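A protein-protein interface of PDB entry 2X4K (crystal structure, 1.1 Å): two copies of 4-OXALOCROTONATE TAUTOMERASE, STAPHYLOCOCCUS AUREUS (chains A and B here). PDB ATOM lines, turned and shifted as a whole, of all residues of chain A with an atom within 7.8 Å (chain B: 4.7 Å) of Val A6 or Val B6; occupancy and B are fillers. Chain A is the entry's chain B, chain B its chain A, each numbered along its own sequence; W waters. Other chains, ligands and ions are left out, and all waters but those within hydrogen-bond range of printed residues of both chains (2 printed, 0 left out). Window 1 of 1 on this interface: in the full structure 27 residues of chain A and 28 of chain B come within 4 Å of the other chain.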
ATOM      1  N   MET A   3      -4.175 -23.600 -26.285  1.00  0.00           N
ATOM      2  CA  MET A   3      -4.673 -22.602 -25.325  1.00  0.00           C
ATOM      3  C   MET A   3      -5.192 -21.269 -25.902  1.00  0.00           C
ATOM      4  O   MET A   3      -4.694 -20.201 -25.535  1.00  0.00           O
ATOM      5  CB  MET A   3      -3.608 -22.332 -24.248  1.00  0.00           C
ATOM      6  CG  MET A   3      -4.190 -21.788 -22.941  1.00  0.00           C
ATOM      7  SD  MET A   3      -2.966 -21.333 -21.694  1.00  0.00           S
ATOM      8  CE  MET A   3      -2.523 -19.677 -22.206  1.00  0.00           C
ATOM      9  N   PRO A   4      -6.225 -21.314 -26.766  1.00  0.00           N
ATOM     10  CA  PRO A   4      -6.710 -20.031 -27.264  1.00  0.00           C
ATOM     11  C   PRO A   4      -7.342 -19.170 -26.180  1.00  0.00           C
ATOM     12  O   PRO A   4      -8.094 -19.659 -25.325  1.00  0.00           O
ATOM     13  CB  PRO A   4      -7.757 -20.428 -28.315  1.00  0.00           C
ATOM     14  CG  PRO A   4      -7.397 -21.801 -28.711  1.00  0.00           C
ATOM     15  CD  PRO A   4      -6.949 -22.423 -27.404  1.00  0.00           C
ATOM     16  N   ILE A   5      -7.009 -17.889 -26.215  1.00  0.00           N
ATOM     17  CA  ILE A   5      -7.640 -16.899 -25.348  1.00  0.00           C
ATOM     18  C   ILE A   5      -8.240 -15.823 -26.237  1.00  0.00           C
ATOM     19  O   ILE A   5      -7.510 -15.139 -26.972  1.00  0.00           O
ATOM     20  CB  ILE A   5      -6.639 -16.254 -24.389  1.00  0.00           C
ATOM     21  CG1 ILE A   5      -6.014 -17.312 -23.483  1.00  0.00           C
ATOM     22  CG2 ILE A   5      -7.323 -15.181 -23.536  1.00  0.00           C
ATOM     23  CD1 ILE A   5      -4.901 -16.792 -22.616  1.00  0.00           C
ATOM     24  N   VAL A   6      -9.566 -15.696 -26.175  1.00  0.00           N
ATOM     25  CA  VAL A   6     -10.291 -14.756 -27.006  1.00  0.00           C
ATOM     26  C   VAL A   6     -10.828 -13.636 -26.136  1.00  0.00           C
ATOM     27  O   VAL A   6     -11.511 -13.884 -25.151  1.00  0.00           O
ATOM     28  CB  VAL A   6     -11.475 -15.437 -27.732  1.00  0.00           C
ATOM     29  CG1 VAL A   6     -12.149 -14.457 -28.665  1.00  0.00           C
ATOM     30  CG2 VAL A   6     -11.016 -16.680 -28.494  1.00  0.00           C
ATOM     31  N   ASN A   7     -10.501 -12.405 -26.497  1.00  0.00           N
ATOM     32  CA  ASN A   7     -11.048 -11.221 -25.856  1.00  0.00           C
ATOM     33  C   ASN A   7     -12.041 -10.582 -26.814  1.00  0.00           C
ATOM     34  O   ASN A   7     -11.731 -10.387 -27.976  1.00  0.00           O
ATOM     35  CB  ASN A   7      -9.929 -10.224 -25.542  1.00  0.00           C
ATOM     36  CG  ASN A   7     -10.331  -9.208 -24.511  1.00  0.00           C
ATOM     37  OD1 ASN A   7     -10.400  -9.513 -23.320  1.00  0.00           O
ATOM     38  ND2 ASN A   7     -10.588  -7.989 -24.958  1.00  0.00           N
ATOM     39  N   VAL A   8     -13.238 -10.275 -26.330  1.00  0.00           N
ATOM     40  CA  VAL A   8     -14.239  -9.594 -27.137  1.00  0.00           C
ATOM     41  C   VAL A   8     -14.618  -8.301 -26.439  1.00  0.00           C
ATOM     42  O   VAL A   8     -15.207  -8.319 -25.355  1.00  0.00           O
ATOM     43  CB  VAL A   8     -15.510 -10.446 -27.342  1.00  0.00           C
ATOM     44  CG1 VAL A   8     -16.505  -9.722 -28.256  1.00  0.00           C
ATOM     45  CG2 VAL A   8     -15.157 -11.809 -27.899  1.00  0.00           C
ATOM     46  N   LYS A   9     -14.284  -7.180 -27.064  1.00  0.00           N
ATOM     47  CA  LYS A   9     -14.709  -5.867 -26.596  1.00  0.00           C
ATOM     48  C   LYS A   9     -15.991  -5.517 -27.321  1.00  0.00           C
ATOM     49  O   LYS A   9     -16.029  -5.550 -28.552  1.00  0.00           O
ATOM     50  CB  LYS A   9     -13.647  -4.804 -26.903  1.00  0.00           C
ATOM     51  CG  LYS A   9     -12.338  -4.995 -26.157  1.00  0.00           C
ATOM     52  CD  LYS A   9     -11.253  -4.060 -26.682  1.00  0.00           C
ATOM     53  CE  LYS A   9      -9.879  -4.388 -26.120  1.00  0.00           C
ATOM     54  NZ  LYS A   9      -9.648  -3.800 -24.787  1.00  0.00           N
ATOM     55  N   LEU A  10     -17.045  -5.185 -26.592  1.00  0.00           N
ATOM     56  CA  LEU A  10     -18.268  -4.748 -27.264  1.00  0.00           C
ATOM     57  C   LEU A  10     -19.077  -3.849 -26.346  1.00  0.00           C
ATOM     58  O   LEU A  10     -18.935  -3.869 -25.124  1.00  0.00           O
ATOM     59  CB  LEU A  10     -19.102  -5.924 -27.814  1.00  0.00           C
ATOM     60  CG  LEU A  10     -20.130  -6.561 -26.877  1.00  0.00           C
ATOM     61  CD1 LEU A  10     -20.986  -7.605 -27.568  1.00  0.00           C
ATOM     62  CD2 LEU A  10     -19.396  -7.159 -25.681  1.00  0.00           C
ATOM     63  N   LEU A  22     -22.706 -15.897 -26.766  1.00  0.00           N
ATOM     64  CA  LEU A  22     -21.473 -15.403 -27.368  1.00  0.00           C
ATOM     65  C   LEU A  22     -20.271 -16.269 -26.964  1.00  0.00           C
ATOM     66  O   LEU A  22     -19.474 -16.677 -27.811  1.00  0.00           O
ATOM     67  CB  LEU A  22     -21.255 -13.942 -26.984  1.00  0.00           C
ATOM     68  CG  LEU A  22     -19.973 -13.262 -27.450  1.00  0.00           C
ATOM     69  CD1 LEU A  22     -19.861 -13.247 -28.948  1.00  0.00           C
ATOM     70  CD2 LEU A  22     -19.945 -11.836 -26.910  1.00  0.00           C
ATOM     71  N   VAL A  26     -18.413 -18.378 -29.889  1.00  0.00           N
ATOM     72  CA  VAL A  26     -17.014 -18.084 -30.167  1.00  0.00           C
ATOM     73  C   VAL A  26     -16.175 -19.340 -29.913  1.00  0.00           C
ATOM     74  O   VAL A  26     -15.271 -19.651 -30.679  1.00  0.00           O
ATOM     75  CB  VAL A  26     -16.531 -16.882 -29.337  1.00  0.00           C
ATOM     76  CG1 VAL A  26     -15.028 -16.770 -29.390  1.00  0.00           C
ATOM     77  CG2 VAL A  26     -17.196 -15.602 -29.835  1.00  0.00           C
ATOM     78  N   THR A  27     -16.497 -20.069 -28.853  1.00  0.00           N
ATOM     79  CA  THR A  27     -15.791 -21.310 -28.559  1.00  0.00           C
ATOM     80  C   THR A  27     -15.982 -22.321 -29.696  1.00  0.00           C
ATOM     81  O   THR A  27     -15.018 -22.929 -30.163  1.00  0.00           O
ATOM     82  CB  THR A  27     -16.247 -21.885 -27.220  1.00  0.00           C
ATOM     83  OG1 THR A  27     -15.980 -20.927 -26.191  1.00  0.00           O
ATOM     84  CG2 THR A  27     -15.511 -23.170 -26.897  1.00  0.00           C
ATOM     85  N   VAL A  30     -13.781 -21.259 -32.690  1.00  0.00           N
ATOM     86  CA  VAL A  30     -12.367 -21.540 -32.481  1.00  0.00           C
ATOM     87  C   VAL A  30     -12.085 -23.040 -32.593  1.00  0.00           C
ATOM     88  O   VAL A  30     -11.130 -23.454 -33.253  1.00  0.00           O
ATOM     89  CB  VAL A  30     -11.885 -20.992 -31.126  1.00  0.00           C
ATOM     90  CG1 VAL A  30     -10.449 -21.428 -30.842  1.00  0.00           C
ATOM     91  CG2 VAL A  30     -11.975 -19.487 -31.128  1.00  0.00           C
ATOM     92  N   ALA A  40      -9.455 -26.077 -23.540  1.00  0.00           N
ATOM     93  CA  ALA A  40      -8.379 -25.094 -23.547  1.00  0.00           C
ATOM     94  C   ALA A  40      -8.769 -23.761 -24.185  1.00  0.00           C
ATOM     95  O   ALA A  40      -7.910 -22.898 -24.346  1.00  0.00           O
ATOM     96  CB  ALA A  40      -7.174 -25.672 -24.277  1.00  0.00           C
ATOM     97  N   ILE A  41     -10.039 -23.590 -24.562  1.00  0.00           N
ATOM     98  CA  ILE A  41     -10.487 -22.363 -25.228  1.00  0.00           C
ATOM     99  C   ILE A  41     -11.162 -21.450 -24.201  1.00  0.00           C
ATOM    100  O   ILE A  41     -12.117 -21.854 -23.540  1.00  0.00           O
ATOM    101  CB  ILE A  41     -11.472 -22.655 -26.385  1.00  0.00           C
ATOM    102  CG1 ILE A  41     -10.811 -23.522 -27.463  1.00  0.00           C
ATOM    103  CG2 ILE A  41     -11.982 -21.351 -26.981  1.00  0.00           C
ATOM    104  CD1 ILE A  41     -11.796 -24.111 -28.473  1.00  0.00           C
ATOM    105  N   HIS A  42     -10.655 -20.224 -24.088  1.00  0.00           N
ATOM    106  CA  HIS A  42     -11.107 -19.253 -23.100  1.00  0.00           C
ATOM    107  C   HIS A  42     -11.673 -18.042 -23.812  1.00  0.00           C
ATOM    108  O   HIS A  42     -11.106 -17.597 -24.805  1.00  0.00           O
ATOM    109  CB  HIS A  42      -9.924 -18.801 -22.253  1.00  0.00           C
ATOM    110  CG  HIS A  42      -9.142 -19.938 -21.679  1.00  0.00           C
ATOM    111  ND1 HIS A  42      -8.292 -20.715 -22.436  1.00  0.00           N
ATOM    112  CD2 HIS A  42      -9.111 -20.455 -20.428  1.00  0.00           C
ATOM    113  CE1 HIS A  42      -7.767 -21.657 -21.672  1.00  0.00           C
ATOM    114  NE2 HIS A  42      -8.259 -21.530 -20.453  1.00  0.00           N
ATOM    115  N   VAL A  43     -12.768 -17.501 -23.291  1.00  0.00           N
ATOM    116  CA  VAL A  43     -13.382 -16.307 -23.849  1.00  0.00           C
ATOM    117  C   VAL A  43     -13.629 -15.310 -22.723  1.00  0.00           C
ATOM    118  O   VAL A  43     -14.189 -15.666 -21.688  1.00  0.00           O
ATOM    119  CB  VAL A  43     -14.704 -16.631 -24.558  1.00  0.00           C
ATOM    120  CG1 VAL A  43     -15.293 -15.376 -25.185  1.00  0.00           C
ATOM    121  CG2 VAL A  43     -14.492 -17.716 -25.616  1.00  0.00           C
ATOM    122  N   VAL A  44     -13.209 -14.062 -22.925  1.00  0.00           N
ATOM    123  CA  VAL A  44     -13.446 -12.970 -21.984  1.00  0.00           C
ATOM    124  C   VAL A  44     -14.162 -11.859 -22.737  1.00  0.00           C
ATOM    125  O   VAL A  44     -13.727 -11.454 -23.812  1.00  0.00           O
ATOM    126  CB  VAL A  44     -12.137 -12.402 -21.392  1.00  0.00           C
ATOM    127  CG1 VAL A  44     -12.429 -11.211 -20.477  1.00  0.00           C
ATOM    128  CG2 VAL A  44     -11.383 -13.476 -20.649  1.00  0.00           C
ATOM    129  N   ILE A  45     -15.265 -11.385 -22.176  1.00  0.00           N
ATOM    130  CA  ILE A  45     -16.036 -10.292 -22.753  1.00  0.00           C
ATOM    131  C   ILE A  45     -15.793  -9.038 -21.915  1.00  0.00           C
ATOM    132  O   ILE A  45     -16.001  -9.028 -20.706  1.00  0.00           O
ATOM    133  CB  ILE A  45     -17.549 -10.625 -22.809  1.00  0.00           C
ATOM    134  CG1 ILE A  45     -17.770 -11.917 -23.610  1.00  0.00           C
ATOM    135  CG2 ILE A  45     -18.330  -9.468 -23.447  1.00  0.00           C
ATOM    136  CD1 ILE A  45     -19.093 -12.578 -23.364  1.00  0.00           C
ATOM    137  N   GLU A  46     -15.327  -7.988 -22.579  1.00  0.00           N
ATOM    138  CA  GLU A  46     -15.087  -6.700 -21.954  1.00  0.00           C
ATOM    139  C   GLU A  46     -16.088  -5.721 -22.509  1.00  0.00           C
ATOM    140  O   GLU A  46     -16.137  -5.502 -23.708  1.00  0.00           O
ATOM    141  CB  GLU A  46     -13.692  -6.199 -22.278  1.00  0.00           C
ATOM    142  CG  GLU A  46     -12.600  -7.014 -21.656  1.00  0.00           C
ATOM    143  CD  GLU A  46     -11.252  -6.338 -21.771  1.00  0.00           C
ATOM    144  OE1 GLU A  46     -10.896  -5.874 -22.875  1.00  0.00           O
ATOM    145  OE2 GLU A  46     -10.537  -6.259 -20.753  1.00  0.00           O
ATOM    146  N   PRO B   4     -17.800  -4.455 -32.241  1.00  0.00           N
ATOM    147  CA  PRO B   4     -17.015  -5.479 -31.568  1.00  0.00           C
ATOM    148  C   PRO B   4     -15.572  -5.581 -32.079  1.00  0.00           C
ATOM    149  O   PRO B   4     -15.318  -5.518 -33.286  1.00  0.00           O
ATOM    150  CB  PRO B   4     -17.791  -6.766 -31.856  1.00  0.00           C
ATOM    151  CG  PRO B   4     -19.187  -6.314 -32.124  1.00  0.00           C
ATOM    152  CD  PRO B   4     -18.997  -5.032 -32.874  1.00  0.00           C
ATOM    153  N   ILE B   5     -14.641  -5.707 -31.143  1.00  0.00           N
ATOM    154  CA  ILE B   5     -13.239  -5.912 -31.447  1.00  0.00           C
ATOM    155  C   ILE B   5     -12.817  -7.186 -30.752  1.00  0.00           C
ATOM    156  O   ILE B   5     -12.854  -7.270 -29.528  1.00  0.00           O
ATOM    157  CB  ILE B   5     -12.398  -4.747 -30.954  1.00  0.00           C
ATOM    158  CG1 ILE B   5     -12.850  -3.478 -31.665  1.00  0.00           C
ATOM    159  CG2 ILE B   5     -10.917  -5.010 -31.192  1.00  0.00           C
ATOM    160  CD1 ILE B   5     -12.080  -2.269 -31.274  1.00  0.00           C
ATOM    161  N   VAL B   6     -12.434  -8.173 -31.550  1.00  0.00           N
ATOM    162  CA  VAL B   6     -12.079  -9.479 -31.062  1.00  0.00           C
ATOM    163  C   VAL B   6     -10.586  -9.672 -31.225  1.00  0.00           C
ATOM    164  O   VAL B   6     -10.027  -9.382 -32.285  1.00  0.00           O
ATOM    165  CB  VAL B   6     -12.814 -10.561 -31.860  1.00  0.00           C
ATOM    166  CG1 VAL B   6     -12.530 -11.932 -31.280  1.00  0.00           C
ATOM    167  CG2 VAL B   6     -14.305 -10.292 -31.873  1.00  0.00           C
ATOM    168  N   ASN B   7      -9.946 -10.145 -30.163  1.00  0.00           N
ATOM    169  CA  ASN B   7      -8.545 -10.496 -30.186  1.00  0.00           C
ATOM    170  C   ASN B   7      -8.435 -11.980 -29.865  1.00  0.00           C
ATOM    171  O   ASN B   7      -8.995 -12.441 -28.869  1.00  0.00           O
ATOM    172  CB  ASN B   7      -7.792  -9.671 -29.149  1.00  0.00           C
ATOM    173  CG  ASN B   7      -6.303  -9.751 -29.319  1.00  0.00           C
ATOM    174  OD1 ASN B   7      -5.632 -10.531 -28.644  1.00  0.00           O
ATOM    175  ND2 ASN B   7      -5.769  -8.945 -30.234  1.00  0.00           N
ATOM    176  N   VAL B   8      -7.758 -12.732 -30.724  1.00  0.00           N
ATOM    177  CA  VAL B   8      -7.575 -14.156 -30.501  1.00  0.00           C
ATOM    178  C   VAL B   8      -6.087 -14.440 -30.357  1.00  0.00           C
ATOM    179  O   VAL B   8      -5.328 -14.273 -31.306  1.00  0.00           O
ATOM    180  CB  VAL B   8      -8.112 -15.011 -31.668  1.00  0.00           C
ATOM    181  CG1 VAL B   8      -7.955 -16.495 -31.334  1.00  0.00           C
ATOM    182  CG2 VAL B   8      -9.557 -14.670 -31.983  1.00  0.00           C
ATOM    183  N   VAL B  26     -15.556 -16.730 -36.331  1.00  0.00           N
ATOM    184  CA  VAL B  26     -15.655 -15.923 -35.117  1.00  0.00           C
ATOM    185  C   VAL B  26     -16.563 -14.718 -35.377  1.00  0.00           C
ATOM    186  O   VAL B  26     -17.362 -14.325 -34.523  1.00  0.00           O
ATOM    187  CB  VAL B  26     -14.264 -15.479 -34.616  1.00  0.00           C
ATOM    188  CG1 VAL B  26     -14.382 -14.325 -33.627  1.00  0.00           C
ATOM    189  CG2 VAL B  26     -13.520 -16.661 -33.989  1.00  0.00           C
ATOM    190  N   VAL B  30     -20.043 -13.784 -33.323  1.00  0.00           N
ATOM    191  CA  VAL B  30     -20.308 -12.499 -32.683  1.00  0.00           C
ATOM    192  C   VAL B  30     -21.595 -11.898 -33.253  1.00  0.00           C
ATOM    193  O   VAL B  30     -22.471 -11.444 -32.514  1.00  0.00           O
ATOM    194  CB  VAL B  30     -19.123 -11.537 -32.871  1.00  0.00           C
ATOM    195  CG1 VAL B  30     -19.484 -10.132 -32.386  1.00  0.00           C
ATOM    196  CG2 VAL B  30     -17.896 -12.069 -32.129  1.00  0.00           C
ATOM    197  N   HIS B  42     -14.592  -6.640 -35.891  1.00  0.00           N
ATOM    198  CA  HIS B  42     -13.174  -6.662 -36.216  1.00  0.00           C
ATOM    199  C   HIS B  42     -12.507  -7.812 -35.489  1.00  0.00           C
ATOM    200  O   HIS B  42     -12.803  -8.046 -34.319  1.00  0.00           O
ATOM    201  CB  HIS B  42     -12.539  -5.352 -35.772  1.00  0.00           C
ATOM    202  CG  HIS B  42     -13.267  -4.151 -36.270  1.00  0.00           C
ATOM    203  ND1 HIS B  42     -14.435  -3.701 -35.699  1.00  0.00           N
ATOM    204  CD2 HIS B  42     -13.009  -3.319 -37.304  1.00  0.00           C
ATOM    205  CE1 HIS B  42     -14.857  -2.631 -36.347  1.00  0.00           C
ATOM    206  NE2 HIS B  42     -14.014  -2.382 -37.330  1.00  0.00           N
ATOM    207  N   VAL B  43     -11.596  -8.507 -36.163  1.00  0.00           N
ATOM    208  CA  VAL B  43     -10.883  -9.622 -35.560  1.00  0.00           C
ATOM    209  C   VAL B  43      -9.390  -9.466 -35.788  1.00  0.00           C
ATOM    210  O   VAL B  43      -8.949  -9.204 -36.906  1.00  0.00           O
ATOM    211  CB  VAL B  43     -11.355 -10.979 -36.117  1.00  0.00           C
ATOM    212  CG1 VAL B  43     -10.591 -12.136 -35.461  1.00  0.00           C
ATOM    213  CG2 VAL B  43     -12.849 -11.138 -35.927  1.00  0.00           C
ATOM    214  N   VAL B  44      -8.620  -9.633 -34.720  1.00  0.00           N
ATOM    215  CA  VAL B  44      -7.172  -9.669 -34.777  1.00  0.00           C
ATOM    216  C   VAL B  44      -6.695 -10.980 -34.180  1.00  0.00           C
ATOM    217  O   VAL B  44      -7.171 -11.382 -33.122  1.00  0.00           O
ATOM    218  CB  VAL B  44      -6.555  -8.501 -33.989  1.00  0.00           C
ATOM    219  CG1 VAL B  44      -5.033  -8.626 -33.921  1.00  0.00           C
ATOM    220  CG2 VAL B  44      -6.983  -7.163 -34.600  1.00  0.00           C
HETATM  221  O   HOH W   1     -10.426  -7.419 -27.832  1.00  0.00           O
HETATM  222  O   HOH W   2      -6.853 -12.323 -26.588  1.00  0.00           O
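Water W2 bridges the backbone carbonyl oxygen (O) of Ile A5 (2.9 Å) and the side-chain amide oxygen (OD1) of Asn B7 (3.0 Å). Water W1 lies within hydrogen-bond range of ND2 of Asn A7 (2.9 Å) and O of Ile B5 (3.0 Å).
The backbone carbonyl oxygen of Asn B7 lies within hydrogen-bond range of the backbone NH of Asn A7. The backbone NH (N) of Lys A9 is in hydrogen-bond range of the backbone carbonyl oxygen (O) of Ile B5, 2.9 Å away.
Printed residues of chain B within 4 Å of Ile A5: Asn B7 (3.6 Å) and Val B8 (3.7 Å). Val A6 touches just these residues of chain B: Val B6 (3.7 Å) and Asn B7 (3.2 Å). Leu A10 touches none of the printed residues of chain B. Val A26 touches none of the printed residues of chain B. Printed residues of chain A within 4 Å of Pro B4: Lys A9 (3.2 Å). Of the printed residues of chain A, Val B8 touches Ile A5 (3.7 Å). Of the printed residues of chain A, Val B30 touches Leu A22 (3.8 Å).
O of Pro B4 lies within hydrogen-bond range of N of His B42, at 2.9 Å. The backbone NH (N) of Val B6 is in hydrogen-bond range of the backbone carbonyl oxygen (O) of His B42 (2.8 Å). The backbone NH (N) of Val B8 sits at hydrogen-bond distance from the backbone carbonyl oxygen (O) of Val B44 (2.8 Å). The backbone NH (N) of Val A44 lies within hydrogen-bond range of the backbone carbonyl oxygen (O) of Val A6 (2.8 Å). O of Val B6 sits at hydrogen-bond distance from N of Val B44 (2.8 Å). The backbone NH (N) of Val A8 sits at hydrogen-bond distance from the backbone carbonyl oxygen (O) of Val A44.
Ile A5 touches Val B8, and with the chains exchanged Val A8 touches Ile B5. Val A6 touches its own counterpart, Val B6. Val A6 touches Asn B7, and with the chains exchanged Asn A7 touches Val B6. Asn A7 touches its own counterpart, Asn B7. Of the 11 pairs that touch across the chains among the printed residues, 8 have their exchanged pair printed and touching as well.
Among the printed residues, pairs that only touch across the chains: Lys A9 with Pro B4, Asn A7 with Val B6, Val A6 with Asn B7, Val A8 with Ile B5, Ile A5 with Asn B7, Val A6 with Val B6, Asn A7 with Ile B5, Ile A5 with Val B8 and Leu A22 with Val B30.
Along chain A the printed residues that touch a printed residue of chain B span positions 5 to 22. Hydrophobic or aromatic side chains of chain B within 4 Å of the printed part of chain A: Pro B4, Val B6 and Val B30. Along chain B the printed residues that touch a printed residue of chain A span positions 4 to 30.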
